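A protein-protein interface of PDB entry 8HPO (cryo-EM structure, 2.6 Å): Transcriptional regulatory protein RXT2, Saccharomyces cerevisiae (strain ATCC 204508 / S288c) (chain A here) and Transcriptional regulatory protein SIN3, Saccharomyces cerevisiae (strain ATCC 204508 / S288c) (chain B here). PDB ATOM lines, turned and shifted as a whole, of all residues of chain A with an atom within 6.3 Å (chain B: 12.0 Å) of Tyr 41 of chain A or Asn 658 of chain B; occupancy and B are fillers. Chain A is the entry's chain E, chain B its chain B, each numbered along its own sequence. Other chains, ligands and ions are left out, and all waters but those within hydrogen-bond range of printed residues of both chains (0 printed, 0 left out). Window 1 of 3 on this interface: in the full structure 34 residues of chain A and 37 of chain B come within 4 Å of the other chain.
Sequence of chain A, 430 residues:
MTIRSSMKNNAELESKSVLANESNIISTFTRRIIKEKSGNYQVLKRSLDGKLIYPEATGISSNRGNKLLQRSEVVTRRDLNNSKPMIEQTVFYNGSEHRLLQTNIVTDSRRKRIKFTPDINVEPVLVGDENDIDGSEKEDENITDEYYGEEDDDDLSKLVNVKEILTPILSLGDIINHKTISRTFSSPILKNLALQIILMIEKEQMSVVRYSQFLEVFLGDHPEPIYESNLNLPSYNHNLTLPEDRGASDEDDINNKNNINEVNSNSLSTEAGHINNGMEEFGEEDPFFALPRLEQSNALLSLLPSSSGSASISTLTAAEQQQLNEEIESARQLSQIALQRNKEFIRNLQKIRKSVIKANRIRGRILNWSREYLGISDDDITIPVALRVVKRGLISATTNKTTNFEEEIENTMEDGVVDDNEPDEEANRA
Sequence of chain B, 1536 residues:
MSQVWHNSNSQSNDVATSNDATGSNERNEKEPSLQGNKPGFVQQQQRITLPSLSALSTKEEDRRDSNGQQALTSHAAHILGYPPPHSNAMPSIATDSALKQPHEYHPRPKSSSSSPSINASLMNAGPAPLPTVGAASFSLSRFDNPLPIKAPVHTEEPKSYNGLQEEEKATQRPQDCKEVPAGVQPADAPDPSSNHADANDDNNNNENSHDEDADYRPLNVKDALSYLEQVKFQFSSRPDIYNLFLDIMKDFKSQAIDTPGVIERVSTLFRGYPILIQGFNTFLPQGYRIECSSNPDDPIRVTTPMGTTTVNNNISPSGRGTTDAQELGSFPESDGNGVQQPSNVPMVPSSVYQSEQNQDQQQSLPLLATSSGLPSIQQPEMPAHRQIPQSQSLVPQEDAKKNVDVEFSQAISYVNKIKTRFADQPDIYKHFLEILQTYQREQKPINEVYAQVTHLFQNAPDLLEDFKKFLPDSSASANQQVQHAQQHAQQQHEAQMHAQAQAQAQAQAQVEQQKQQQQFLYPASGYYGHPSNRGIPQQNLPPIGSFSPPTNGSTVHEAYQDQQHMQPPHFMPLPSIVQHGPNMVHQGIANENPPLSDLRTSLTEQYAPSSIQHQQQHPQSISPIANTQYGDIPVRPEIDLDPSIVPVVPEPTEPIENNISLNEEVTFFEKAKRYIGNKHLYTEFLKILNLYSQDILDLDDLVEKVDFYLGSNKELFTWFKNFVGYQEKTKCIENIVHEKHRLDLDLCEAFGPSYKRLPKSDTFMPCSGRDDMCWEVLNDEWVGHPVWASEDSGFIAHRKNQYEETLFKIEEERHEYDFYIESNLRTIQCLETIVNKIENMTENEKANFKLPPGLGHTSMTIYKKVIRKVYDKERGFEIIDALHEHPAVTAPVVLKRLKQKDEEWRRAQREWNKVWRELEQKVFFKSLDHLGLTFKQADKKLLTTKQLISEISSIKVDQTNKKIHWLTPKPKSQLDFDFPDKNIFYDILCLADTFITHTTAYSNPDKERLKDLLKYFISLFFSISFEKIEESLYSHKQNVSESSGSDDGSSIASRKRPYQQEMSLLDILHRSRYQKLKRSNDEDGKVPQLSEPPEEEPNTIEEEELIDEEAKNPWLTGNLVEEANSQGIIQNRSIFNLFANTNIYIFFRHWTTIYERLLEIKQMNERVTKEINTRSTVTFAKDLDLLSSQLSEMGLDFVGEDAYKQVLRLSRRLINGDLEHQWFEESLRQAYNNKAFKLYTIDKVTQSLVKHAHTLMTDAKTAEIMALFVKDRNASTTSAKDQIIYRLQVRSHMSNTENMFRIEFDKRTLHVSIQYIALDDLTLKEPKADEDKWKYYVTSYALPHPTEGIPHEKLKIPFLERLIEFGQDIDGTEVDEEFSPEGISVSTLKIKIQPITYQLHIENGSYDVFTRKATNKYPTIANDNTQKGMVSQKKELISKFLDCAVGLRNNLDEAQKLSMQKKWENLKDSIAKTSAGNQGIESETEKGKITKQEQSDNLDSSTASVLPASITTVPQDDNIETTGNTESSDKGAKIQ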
ATOM      1  N   ARG A  31     -18.715 -19.143  -8.403  1.00  0.00           N
ATOM      2  CA  ARG A  31     -19.962 -19.825  -8.727  1.00  0.00           C
ATOM      3  C   ARG A  31     -19.930 -21.271  -8.262  1.00  0.00           C
ATOM      4  O   ARG A  31     -20.881 -21.756  -7.642  1.00  0.00           O
ATOM      5  CB  ARG A  31     -20.221 -19.754 -10.230  1.00  0.00           C
ATOM      6  CG  ARG A  31     -20.938 -18.500 -10.670  1.00  0.00           C
ATOM      7  CD  ARG A  31     -22.435 -18.714 -10.676  1.00  0.00           C
ATOM      8  NE  ARG A  31     -23.018 -18.465  -9.365  1.00  0.00           N
ATOM      9  CZ  ARG A  31     -23.368 -17.263  -8.932  1.00  0.00           C
ATOM     10  NH1 ARG A  31     -23.189 -16.206  -9.708  1.00  0.00           N
ATOM     11  NH2 ARG A  31     -23.897 -17.114  -7.728  1.00  0.00           N
ATOM     12  N   ILE A  34     -20.093 -21.479  -4.415  1.00  0.00           N
ATOM     13  CA  ILE A  34     -21.420 -21.181  -3.888  1.00  0.00           C
ATOM     14  C   ILE A  34     -22.392 -22.312  -4.203  1.00  0.00           C
ATOM     15  O   ILE A  34     -23.237 -22.672  -3.376  1.00  0.00           O
ATOM     16  CB  ILE A  34     -21.913 -19.834  -4.440  1.00  0.00           C
ATOM     17  CG1 ILE A  34     -21.051 -18.705  -3.881  1.00  0.00           C
ATOM     18  CG2 ILE A  34     -23.363 -19.612  -4.084  1.00  0.00           C
ATOM     19  CD1 ILE A  34     -21.652 -17.339  -4.052  1.00  0.00           C
ATOM     20  N   LYS A  35     -22.279 -22.905  -5.391  1.00  0.00           N
ATOM     21  CA  LYS A  35     -23.160 -24.011  -5.736  1.00  0.00           C
ATOM     22  C   LYS A  35     -22.880 -25.243  -4.887  1.00  0.00           C
ATOM     23  O   LYS A  35     -23.820 -25.880  -4.407  1.00  0.00           O
ATOM     24  CB  LYS A  35     -23.035 -24.347  -7.219  1.00  0.00           C
ATOM     25  CG  LYS A  35     -23.809 -23.421  -8.131  1.00  0.00           C
ATOM     26  CD  LYS A  35     -24.261 -24.159  -9.369  1.00  0.00           C
ATOM     27  CE  LYS A  35     -25.239 -23.339 -10.182  1.00  0.00           C
ATOM     28  NZ  LYS A  35     -25.689 -24.066 -11.397  1.00  0.00           N
ATOM     29  N   GLU A  36     -21.611 -25.596  -4.680  1.00  0.00           N
ATOM     30  CA  GLU A  36     -21.326 -26.750  -3.836  1.00  0.00           C
ATOM     31  C   GLU A  36     -21.588 -26.457  -2.364  1.00  0.00           C
ATOM     32  O   GLU A  36     -21.677 -27.390  -1.560  1.00  0.00           O
ATOM     33  CB  GLU A  36     -19.885 -27.219  -4.042  1.00  0.00           C
ATOM     34  CG  GLU A  36     -19.616 -28.659  -3.598  1.00  0.00           C
ATOM     35  CD  GLU A  36     -19.577 -29.654  -4.754  1.00  0.00           C
ATOM     36  OE1 GLU A  36     -18.925 -30.709  -4.612  1.00  0.00           O
ATOM     37  OE2 GLU A  36     -20.208 -29.392  -5.799  1.00  0.00           O
ATOM     38  N   SER A  38     -24.374 -24.702  -1.625  1.00  0.00           N
ATOM     39  CA  SER A  38     -25.827 -24.594  -1.553  1.00  0.00           C
ATOM     40  C   SER A  38     -26.444 -25.694  -0.704  1.00  0.00           C
ATOM     41  O   SER A  38     -27.554 -25.518  -0.195  1.00  0.00           O
ATOM     42  CB  SER A  38     -26.433 -24.631  -2.953  1.00  0.00           C
ATOM     43  OG  SER A  38     -27.774 -25.075  -2.902  1.00  0.00           O
ATOM     44  N   GLY A  39     -25.754 -26.820  -0.545  1.00  0.00           N
ATOM     45  CA  GLY A  39     -26.252 -27.936   0.222  1.00  0.00           C
ATOM     46  C   GLY A  39     -26.776 -29.089  -0.601  1.00  0.00           C
ATOM     47  O   GLY A  39     -27.045 -30.154  -0.042  1.00  0.00           O
ATOM     48  N   ASN A  40     -26.937 -28.906  -1.902  1.00  0.00           N
ATOM     49  CA  ASN A  40     -27.391 -29.940  -2.816  1.00  0.00           C
ATOM     50  C   ASN A  40     -26.223 -30.578  -3.569  1.00  0.00           C
ATOM     51  O   ASN A  40     -25.043 -30.419  -3.248  1.00  0.00           O
ATOM     52  CB  ASN A  40     -28.405 -29.379  -3.819  1.00  0.00           C
ATOM     53  CG  ASN A  40     -29.400 -28.438  -3.184  1.00  0.00           C
ATOM     54  OD1 ASN A  40     -29.691 -28.541  -1.998  1.00  0.00           O
ATOM     55  ND2 ASN A  40     -29.937 -27.520  -3.976  1.00  0.00           N
ATOM     56  N   TYR A  41     -26.624 -31.341  -4.569  1.00  0.00           N
ATOM     57  CA  TYR A  41     -25.929 -31.873  -5.736  1.00  0.00           C
ATOM     58  C   TYR A  41     -25.032 -33.098  -5.606  1.00  0.00           C
ATOM     59  O   TYR A  41     -25.007 -33.877  -6.565  1.00  0.00           O
ATOM     60  CB  TYR A  41     -25.014 -30.785  -6.321  1.00  0.00           C
ATOM     61  CG  TYR A  41     -25.684 -29.506  -6.733  1.00  0.00           C
ATOM     62  CD1 TYR A  41     -26.409 -29.429  -7.908  1.00  0.00           C
ATOM     63  CD2 TYR A  41     -25.580 -28.371  -5.954  1.00  0.00           C
ATOM     64  CE1 TYR A  41     -27.022 -28.260  -8.286  1.00  0.00           C
ATOM     65  CE2 TYR A  41     -26.188 -27.200  -6.323  1.00  0.00           C
ATOM     66  CZ  TYR A  41     -26.909 -27.148  -7.489  1.00  0.00           C
ATOM     67  OH  TYR A  41     -27.519 -25.978  -7.861  1.00  0.00           O
ATOM     68  N   GLN A  42     -24.250 -33.282  -4.533  1.00  0.00           N
ATOM     69  CA  GLN A  42     -23.926 -34.575  -3.927  1.00  0.00           C
ATOM     70  C   GLN A  42     -22.466 -34.552  -3.501  1.00  0.00           C
ATOM     71  O   GLN A  42     -21.816 -33.503  -3.533  1.00  0.00           O
ATOM     72  CB  GLN A  42     -24.213 -35.807  -4.775  1.00  0.00           C
ATOM     73  CG  GLN A  42     -25.326 -36.626  -4.141  1.00  0.00           C
ATOM     74  CD  GLN A  42     -25.100 -36.854  -2.648  1.00  0.00           C
ATOM     75  OE1 GLN A  42     -24.002 -37.207  -2.218  1.00  0.00           O
ATOM     76  NE2 GLN A  42     -26.142 -36.641  -1.853  1.00  0.00           N
ATOM     77  N   VAL A  43     -21.938 -35.708  -3.112  1.00  0.00           N
ATOM     78  CA  VAL A  43     -20.549 -36.046  -3.406  1.00  0.00           C
ATOM     79  C   VAL A  43     -20.488 -37.495  -3.874  1.00  0.00           C
ATOM     80  O   VAL A  43     -20.776 -38.422  -3.112  1.00  0.00           O
ATOM     81  CB  VAL A  43     -19.609 -35.788  -2.211  1.00  0.00           C
ATOM     82  CG1 VAL A  43     -20.083 -36.501  -0.951  1.00  0.00           C
ATOM     83  CG2 VAL A  43     -18.187 -36.202  -2.568  1.00  0.00           C
ATOM     84  N   LEU A  44     -20.133 -37.688  -5.140  1.00  0.00           N
ATOM     85  CA  LEU A  44     -20.057 -39.008  -5.750  1.00  0.00           C
ATOM     86  C   LEU A  44     -18.682 -39.610  -5.516  1.00  0.00           C
ATOM     87  O   LEU A  44     -17.691 -38.886  -5.409  1.00  0.00           O
ATOM     88  CB  LEU A  44     -20.332 -38.941  -7.254  1.00  0.00           C
ATOM     89  CG  LEU A  44     -21.785 -38.968  -7.719  1.00  0.00           C
ATOM     90  CD1 LEU A  44     -21.892 -38.470  -9.147  1.00  0.00           C
ATOM     91  CD2 LEU A  44     -22.339 -40.368  -7.604  1.00  0.00           C
ATOM     92  N   GLN A  89     -33.433 -38.578  -2.379  1.00  0.00           N
ATOM     93  CA  GLN A  89     -32.739 -37.334  -2.062  1.00  0.00           C
ATOM     94  C   GLN A  89     -33.645 -36.112  -2.162  1.00  0.00           C
ATOM     95  O   GLN A  89     -34.611 -36.089  -2.929  1.00  0.00           O
ATOM     96  CB  GLN A  89     -31.554 -37.135  -3.002  1.00  0.00           C
ATOM     97  CG  GLN A  89     -30.467 -38.175  -2.895  1.00  0.00           C
ATOM     98  CD  GLN A  89     -29.118 -37.632  -3.323  1.00  0.00           C
ATOM     99  OE1 GLN A  89     -29.014 -36.505  -3.814  1.00  0.00           O
ATOM    100  NE2 GLN A  89     -28.077 -38.433  -3.145  1.00  0.00           N
ATOM    101  N   THR A  90     -33.312 -35.087  -1.385  1.00  0.00           N
ATOM    102  CA  THR A  90     -34.118 -33.883  -1.253  1.00  0.00           C
ATOM    103  C   THR A  90     -33.331 -32.698  -1.802  1.00  0.00           C
ATOM    104  O   THR A  90     -32.103 -32.755  -1.892  1.00  0.00           O
ATOM    105  CB  THR A  90     -34.488 -33.650   0.215  1.00  0.00           C
ATOM    106  OG1 THR A  90     -35.064 -34.845   0.757  1.00  0.00           O
ATOM    107  CG2 THR A  90     -35.509 -32.546   0.342  1.00  0.00           C
ATOM    108  N   VAL A  91     -34.035 -31.632  -2.165  1.00  0.00           N
ATOM    109  CA  VAL A  91     -33.436 -30.468  -2.800  1.00  0.00           C
ATOM    110  C   VAL A  91     -34.250 -29.234  -2.435  1.00  0.00           C
ATOM    111  O   VAL A  91     -35.478 -29.244  -2.541  1.00  0.00           O
ATOM    112  CB  VAL A  91     -33.353 -30.653  -4.325  1.00  0.00           C
ATOM    113  CG1 VAL A  91     -33.560 -29.345  -5.043  1.00  0.00           C
ATOM    114  CG2 VAL A  91     -32.018 -31.248  -4.702  1.00  0.00           C
ATOM    115  N   PHE A  92     -33.569 -28.179  -2.003  1.00  0.00           N
ATOM    116  CA  PHE A  92     -34.209 -26.900  -1.725  1.00  0.00           C
ATOM    117  C   PHE A  92     -34.298 -26.122  -3.030  1.00  0.00           C
ATOM    118  O   PHE A  92     -33.306 -26.004  -3.752  1.00  0.00           O
ATOM    119  CB  PHE A  92     -33.422 -26.128  -0.671  1.00  0.00           C
ATOM    120  CG  PHE A  92     -34.178 -24.986  -0.066  1.00  0.00           C
ATOM    121  CD1 PHE A  92     -34.270 -23.774  -0.725  1.00  0.00           C
ATOM    122  CD2 PHE A  92     -34.798 -25.124   1.159  1.00  0.00           C
ATOM    123  CE1 PHE A  92     -34.967 -22.726  -0.176  1.00  0.00           C
ATOM    124  CE2 PHE A  92     -35.493 -24.081   1.711  1.00  0.00           C
ATOM    125  CZ  PHE A  92     -35.578 -22.878   1.042  1.00  0.00           C
ATOM    126  N   THR B 653     -39.744 -20.751 -16.080  1.00  0.00           N
ATOM    127  CA  THR B 653     -39.215 -21.211 -14.802  1.00  0.00           C
ATOM    128  C   THR B 653     -38.649 -19.995 -14.085  1.00  0.00           C
ATOM    129  O   THR B 653     -38.368 -18.968 -14.708  1.00  0.00           O
ATOM    130  CB  THR B 653     -38.130 -22.290 -14.977  1.00  0.00           C
ATOM    131  OG1 THR B 653     -38.668 -23.411 -15.685  1.00  0.00           O
ATOM    132  CG2 THR B 653     -37.620 -22.781 -13.651  1.00  0.00           C
ATOM    133  N   GLU B 654     -38.481 -20.121 -12.770  1.00  0.00           N
ATOM    134  CA  GLU B 654     -37.685 -19.188 -11.991  1.00  0.00           C
ATOM    135  C   GLU B 654     -36.326 -19.812 -11.729  1.00  0.00           C
ATOM    136  O   GLU B 654     -36.260 -20.913 -11.165  1.00  0.00           O
ATOM    137  CB  GLU B 654     -38.380 -18.845 -10.676  1.00  0.00           C
ATOM    138  CG  GLU B 654     -39.772 -18.256 -10.840  1.00  0.00           C
ATOM    139  CD  GLU B 654     -39.763 -16.799 -11.271  1.00  0.00           C
ATOM    140  OE1 GLU B 654     -38.872 -16.393 -12.047  1.00  0.00           O
ATOM    141  OE2 GLU B 654     -40.659 -16.051 -10.830  1.00  0.00           O
ATOM    142  N   PRO B 655     -35.233 -19.171 -12.135  1.00  0.00           N
ATOM    143  CA  PRO B 655     -33.907 -19.753 -11.908  1.00  0.00           C
ATOM    144  C   PRO B 655     -33.603 -19.868 -10.427  1.00  0.00           C
ATOM    145  O   PRO B 655     -34.132 -19.132  -9.593  1.00  0.00           O
ATOM    146  CB  PRO B 655     -32.956 -18.764 -12.593  1.00  0.00           C
ATOM    147  CG  PRO B 655     -33.812 -17.991 -13.537  1.00  0.00           C
ATOM    148  CD  PRO B 655     -35.158 -17.909 -12.885  1.00  0.00           C
ATOM    149  N   ILE B 656     -32.719 -20.813 -10.110  1.00  0.00           N
ATOM    150  CA  ILE B 656     -32.408 -21.087  -8.720  1.00  0.00           C
ATOM    151  C   ILE B 656     -31.730 -19.877  -8.083  1.00  0.00           C
ATOM    152  O   ILE B 656     -31.274 -18.951  -8.762  1.00  0.00           O
ATOM    153  CB  ILE B 656     -31.524 -22.337  -8.614  1.00  0.00           C
ATOM    154  CG1 ILE B 656     -31.784 -23.250  -9.804  1.00  0.00           C
ATOM    155  CG2 ILE B 656     -31.809 -23.084  -7.332  1.00  0.00           C
ATOM    156  CD1 ILE B 656     -30.901 -24.453  -9.816  1.00  0.00           C
ATOM    157  N   GLU B 657     -31.681 -19.882  -6.753  1.00  0.00           N
ATOM    158  CA  GLU B 657     -31.110 -18.777  -5.998  1.00  0.00           C
ATOM    159  C   GLU B 657     -29.593 -18.725  -6.055  1.00  0.00           C
ATOM    160  O   GLU B 657     -29.034 -17.627  -6.107  1.00  0.00           O
ATOM    161  CB  GLU B 657     -31.546 -18.849  -4.533  1.00  0.00           C
ATOM    162  CG  GLU B 657     -32.629 -17.853  -4.167  1.00  0.00           C
ATOM    163  CD  GLU B 657     -32.586 -16.607  -5.029  1.00  0.00           C
ATOM    164  OE1 GLU B 657     -33.459 -16.461  -5.910  1.00  0.00           O
ATOM    165  OE2 GLU B 657     -31.680 -15.772  -4.827  1.00  0.00           O
ATOM    166  N   ASN B 658     -28.914 -19.867  -6.069  1.00  0.00           N
ATOM    167  CA  ASN B 658     -27.463 -19.882  -5.972  1.00  0.00           C
ATOM    168  C   ASN B 658     -26.785 -19.594  -7.299  1.00  0.00           C
ATOM    169  O   ASN B 658     -25.622 -19.967  -7.484  1.00  0.00           O
ATOM    170  CB  ASN B 658     -26.978 -21.217  -5.396  1.00  0.00           C
ATOM    171  CG  ASN B 658     -27.280 -22.393  -6.297  1.00  0.00           C
ATOM    172  OD1 ASN B 658     -26.744 -22.504  -7.396  1.00  0.00           O
ATOM    173  ND2 ASN B 658     -28.138 -23.290  -5.825  1.00  0.00           N
ATOM    174  N   ASN B 659     -27.491 -18.963  -8.233  1.00  0.00           N
ATOM    175  CA  ASN B 659     -26.908 -18.548  -9.498  1.00  0.00           C
ATOM    176  C   ASN B 659     -26.671 -17.049  -9.612  1.00  0.00           C
ATOM    177  O   ASN B 659     -25.863 -16.635 -10.443  1.00  0.00           O
ATOM    178  CB  ASN B 659     -27.802 -18.989 -10.663  1.00  0.00           C
ATOM    179  CG  ASN B 659     -27.990 -20.489 -10.717  1.00  0.00           C
ATOM    180  OD1 ASN B 659     -27.673 -21.197  -9.766  1.00  0.00           O
ATOM    181  ND2 ASN B 659     -28.513 -20.982 -11.833  1.00  0.00           N
ATOM    182  N   ILE B 660     -27.356 -16.220  -8.822  1.00  0.00           N
ATOM    183  CA  ILE B 660     -27.326 -14.775  -9.044  1.00  0.00           C
ATOM    184  C   ILE B 660     -26.963 -14.004  -7.774  1.00  0.00           C
ATOM    185  O   ILE B 660     -27.431 -12.880  -7.568  1.00  0.00           O
ATOM    186  CB  ILE B 660     -28.664 -14.268  -9.624  1.00  0.00           C
ATOM    187  CG1 ILE B 660     -29.277 -15.277 -10.599  1.00  0.00           C
ATOM    188  CG2 ILE B 660     -28.459 -12.967 -10.389  1.00  0.00           C
ATOM    189  CD1 ILE B 660     -30.240 -16.253  -9.966  1.00  0.00           C
ATOM    190  N   SER B 661     -26.149 -14.593  -6.897  1.00  0.00           N
ATOM    191  CA  SER B 661     -25.710 -13.912  -5.674  1.00  0.00           C
ATOM    192  C   SER B 661     -24.186 -13.987  -5.582  1.00  0.00           C
ATOM    193  O   SER B 661     -23.644 -14.971  -5.072  1.00  0.00           O
ATOM    194  CB  SER B 661     -26.375 -14.527  -4.441  1.00  0.00           C
ATOM    195  OG  SER B 661     -27.756 -14.750  -4.659  1.00  0.00           O
ATOM    196  N   LEU B 662     -23.488 -12.953  -6.082  1.00  0.00           N
ATOM    197  CA  LEU B 662     -22.030 -13.012  -6.120  1.00  0.00           C
ATOM    198  C   LEU B 662     -21.301 -11.717  -5.761  1.00  0.00           C
ATOM    199  O   LEU B 662     -20.083 -11.757  -5.546  1.00  0.00           O
ATOM    200  CB  LEU B 662     -21.579 -13.466  -7.514  1.00  0.00           C
ATOM    201  CG  LEU B 662     -20.225 -14.162  -7.582  1.00  0.00           C
ATOM    202  CD1 LEU B 662     -20.108 -15.113  -6.416  1.00  0.00           C
ATOM    203  CD2 LEU B 662     -20.061 -14.896  -8.898  1.00  0.00           C
ATOM    204  N   ASN B 663     -21.984 -10.579  -5.661  1.00  0.00           N
ATOM    205  CA  ASN B 663     -21.297  -9.307  -5.870  1.00  0.00           C
ATOM    206  C   ASN B 663     -20.570  -8.763  -4.643  1.00  0.00           C
ATOM    207  O   ASN B 663     -19.850  -7.766  -4.772  1.00  0.00           O
ATOM    208  CB  ASN B 663     -22.293  -8.257  -6.374  1.00  0.00           C
ATOM    209  CG  ASN B 663     -21.615  -7.112  -7.107  1.00  0.00           C
ATOM    210  OD1 ASN B 663     -20.443  -7.201  -7.475  1.00  0.00           O
ATOM    211  ND2 ASN B 663     -22.353  -6.031  -7.327  1.00  0.00           N
ATOM    212  N   TYR B 692      -8.651 -26.132 -10.236  1.00  0.00           N
ATOM    213  CA  TYR B 692      -9.666 -26.699  -9.352  1.00  0.00           C
ATOM    214  C   TYR B 692     -11.056 -26.580  -9.956  1.00  0.00           C
ATOM    215  O   TYR B 692     -11.823 -27.551  -9.964  1.00  0.00           O
ATOM    216  CB  TYR B 692      -9.628 -26.012  -7.994  1.00  0.00           C
ATOM    217  CG  TYR B 692     -10.766 -26.390  -7.077  1.00  0.00           C
ATOM    218  CD1 TYR B 692     -11.859 -25.552  -6.912  1.00  0.00           C
ATOM    219  CD2 TYR B 692     -10.743 -27.582  -6.369  1.00  0.00           C
ATOM    220  CE1 TYR B 692     -12.894 -25.891  -6.072  1.00  0.00           C
ATOM    221  CE2 TYR B 692     -11.774 -27.929  -5.524  1.00  0.00           C
ATOM    222  CZ  TYR B 692     -12.847 -27.079  -5.380  1.00  0.00           C
ATOM    223  OH  TYR B 692     -13.877 -27.424  -4.540  1.00  0.00           O
ATOM    224  N   ASP B 695     -12.369 -29.378 -11.742  1.00  0.00           N
ATOM    225  CA  ASP B 695     -12.381 -30.655 -11.022  1.00  0.00           C
ATOM    226  C   ASP B 695     -11.155 -31.509 -11.333  1.00  0.00           C
ATOM    227  O   ASP B 695     -11.282 -32.646 -11.794  1.00  0.00           O
ATOM    228  CB  ASP B 695     -13.657 -31.450 -11.314  1.00  0.00           C
ATOM    229  CG  ASP B 695     -14.911 -30.609 -11.198  1.00  0.00           C
ATOM    230  OD1 ASP B 695     -15.888 -31.079 -10.576  1.00  0.00           O
ATOM    231  OD2 ASP B 695     -14.924 -29.482 -11.730  1.00  0.00           O
ATOM    232  N   PHE B 723     -14.043 -19.619   3.425  1.00  0.00           N
ATOM    233  CA  PHE B 723     -14.838 -19.485   2.207  1.00  0.00           C
ATOM    234  C   PHE B 723     -15.050 -20.839   1.542  1.00  0.00           C
ATOM    235  O   PHE B 723     -16.188 -21.271   1.334  1.00  0.00           O
ATOM    236  CB  PHE B 723     -14.166 -18.514   1.241  1.00  0.00           C
ATOM    237  CG  PHE B 723     -14.957 -18.261  -0.006  1.00  0.00           C
ATOM    238  CD1 PHE B 723     -14.429 -18.559  -1.247  1.00  0.00           C
ATOM    239  CD2 PHE B 723     -16.228 -17.725   0.064  1.00  0.00           C
ATOM    240  CE1 PHE B 723     -15.151 -18.327  -2.392  1.00  0.00           C
ATOM    241  CE2 PHE B 723     -16.955 -17.491  -1.084  1.00  0.00           C
ATOM    242  CZ  PHE B 723     -16.414 -17.793  -2.313  1.00  0.00           C
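Of the printed residues of chain B, Ile 34 of chain A touches Ser 661 and Leu 662. Of chain B, only Asn 658 (3.2 Å) and Asn 659 (3.3 Å) come within 4 Å of Lys 35 of chain A. Of chain B, only Asn 658 (3.4 Å) comes within 4 Å of Ser 38 of chain A. No residue of chain B comes within 4 Å of Gly 39 of chain A. No residue of chain B comes within 4 Å of Asn 40 of chain A. Tyr 41 of chain A touches just one residue of chain B: Asn 658 (3.4 Å). No residue of chain B comes within 4 Å of Gln 42 of chain A. Leu 44 of chain A touches none of the printed residues of chain B. Asn 658 of chain B touches just these residues of chain A: Arg 31 (3.3 Å), Lys 35 (3.2 Å), Ser 38 (3.4 Å) and Tyr 41 (3.4 Å). Printed residues of chain A within 4 Å of Asn 659 of chain B: Arg 31 and Lys 35. Of the printed residues of chain A, Ile 660 of chain B touches Arg 31 (3.7 Å). Of the printed residues of chain A, Ser 661 of chain B touches Arg 31 (3.4 Å) and Ile 34 (3.3 Å). Of the printed residues of chain A, Leu 662 of chain B touches Arg 31 and Ile 34. Asn 663 of chain B touches none of the printed residues of chain A. The nearest residue of chain A that does not touch Asn 658 of chain B is Ile 34 of chain A (4.1 Å). The nearest printed residue of chain A that does not touch Ile 660 of chain B is Ile 34 of chain A (7.1 Å).
Arg 31 of chain A touches Ile 660 of chain B (NH2 to N, 3.7 Å). CD2 of Leu 662 of chain B touches NH1 of Arg 31 of chain A, 3.5 Å away. CD1 of Ile 34 of chain A touches O of Ser 661 of chain B, at 3.3 Å. Leu 662 of chain B touches Ile 34 of chain A (CD1 to CD1, 3.6 Å). CG of Lys 35 of chain A touches OD1 of Asn 658 of chain B, at 3.2 Å. CE of Lys 35 of chain A touches OD1 of Asn 659 of chain B, at 3.3 Å.
OG of Ser 661 of chain B sits at hydrogen-bond distance from O of Glu 657 of chain B, 3.5 Å away. OG of Ser 38 of chain A is in hydrogen-bond range of ND2 of Asn 40 of chain A (3.4 Å). The side-chain amide oxygen of Asn 658 of chain B sits close to the side-chain amide oxygen of Asn 659 of chain B, 2.9 Å away.
Of the 15 printed residues of chain A, 5 touch a printed residue of chain B. Hydrophobic or aromatic side chains of chain A that line the printed part of chain B: Ile 34 and Tyr 41. Of the 14 printed residues of chain B, 5 touch a printed residue of chain A. Hydrophobic or aromatic side chains of chain B within 4 Å of the printed part of chain A: Leu 662. Along chain B the printed residues that touch a printed residue of chain A span positions 658 to 662. Among the printed residues, no Asp or Glu carboxylate lies within 4 Å of a Lys or Arg side-chain nitrogen of the other chain.
NH1 of Arg 31 of chain A is in hydrogen-bond range of O of Asn 659 of chain B (2.8 Å). NH2 of Arg 31 of chain A lies within hydrogen-bond range of O of Asn 658 of chain B. The side-chain hydroxyl (OG) of Ser 38 of chain A lies within hydrogen-bond range of the side-chain amide nitrogen (ND2) of Asn 658 of chain B (3.4 Å). The guanidinium group (NH2) of Arg 31 of chain A sits at hydrogen-bond distance from the backbone carbonyl oxygen (O) of Ser 661 of chain B (3.4 Å). ND2 of Asn 658 of chain B sits at hydrogen-bond distance from OH of Tyr 41 of chain A (3.4 Å).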
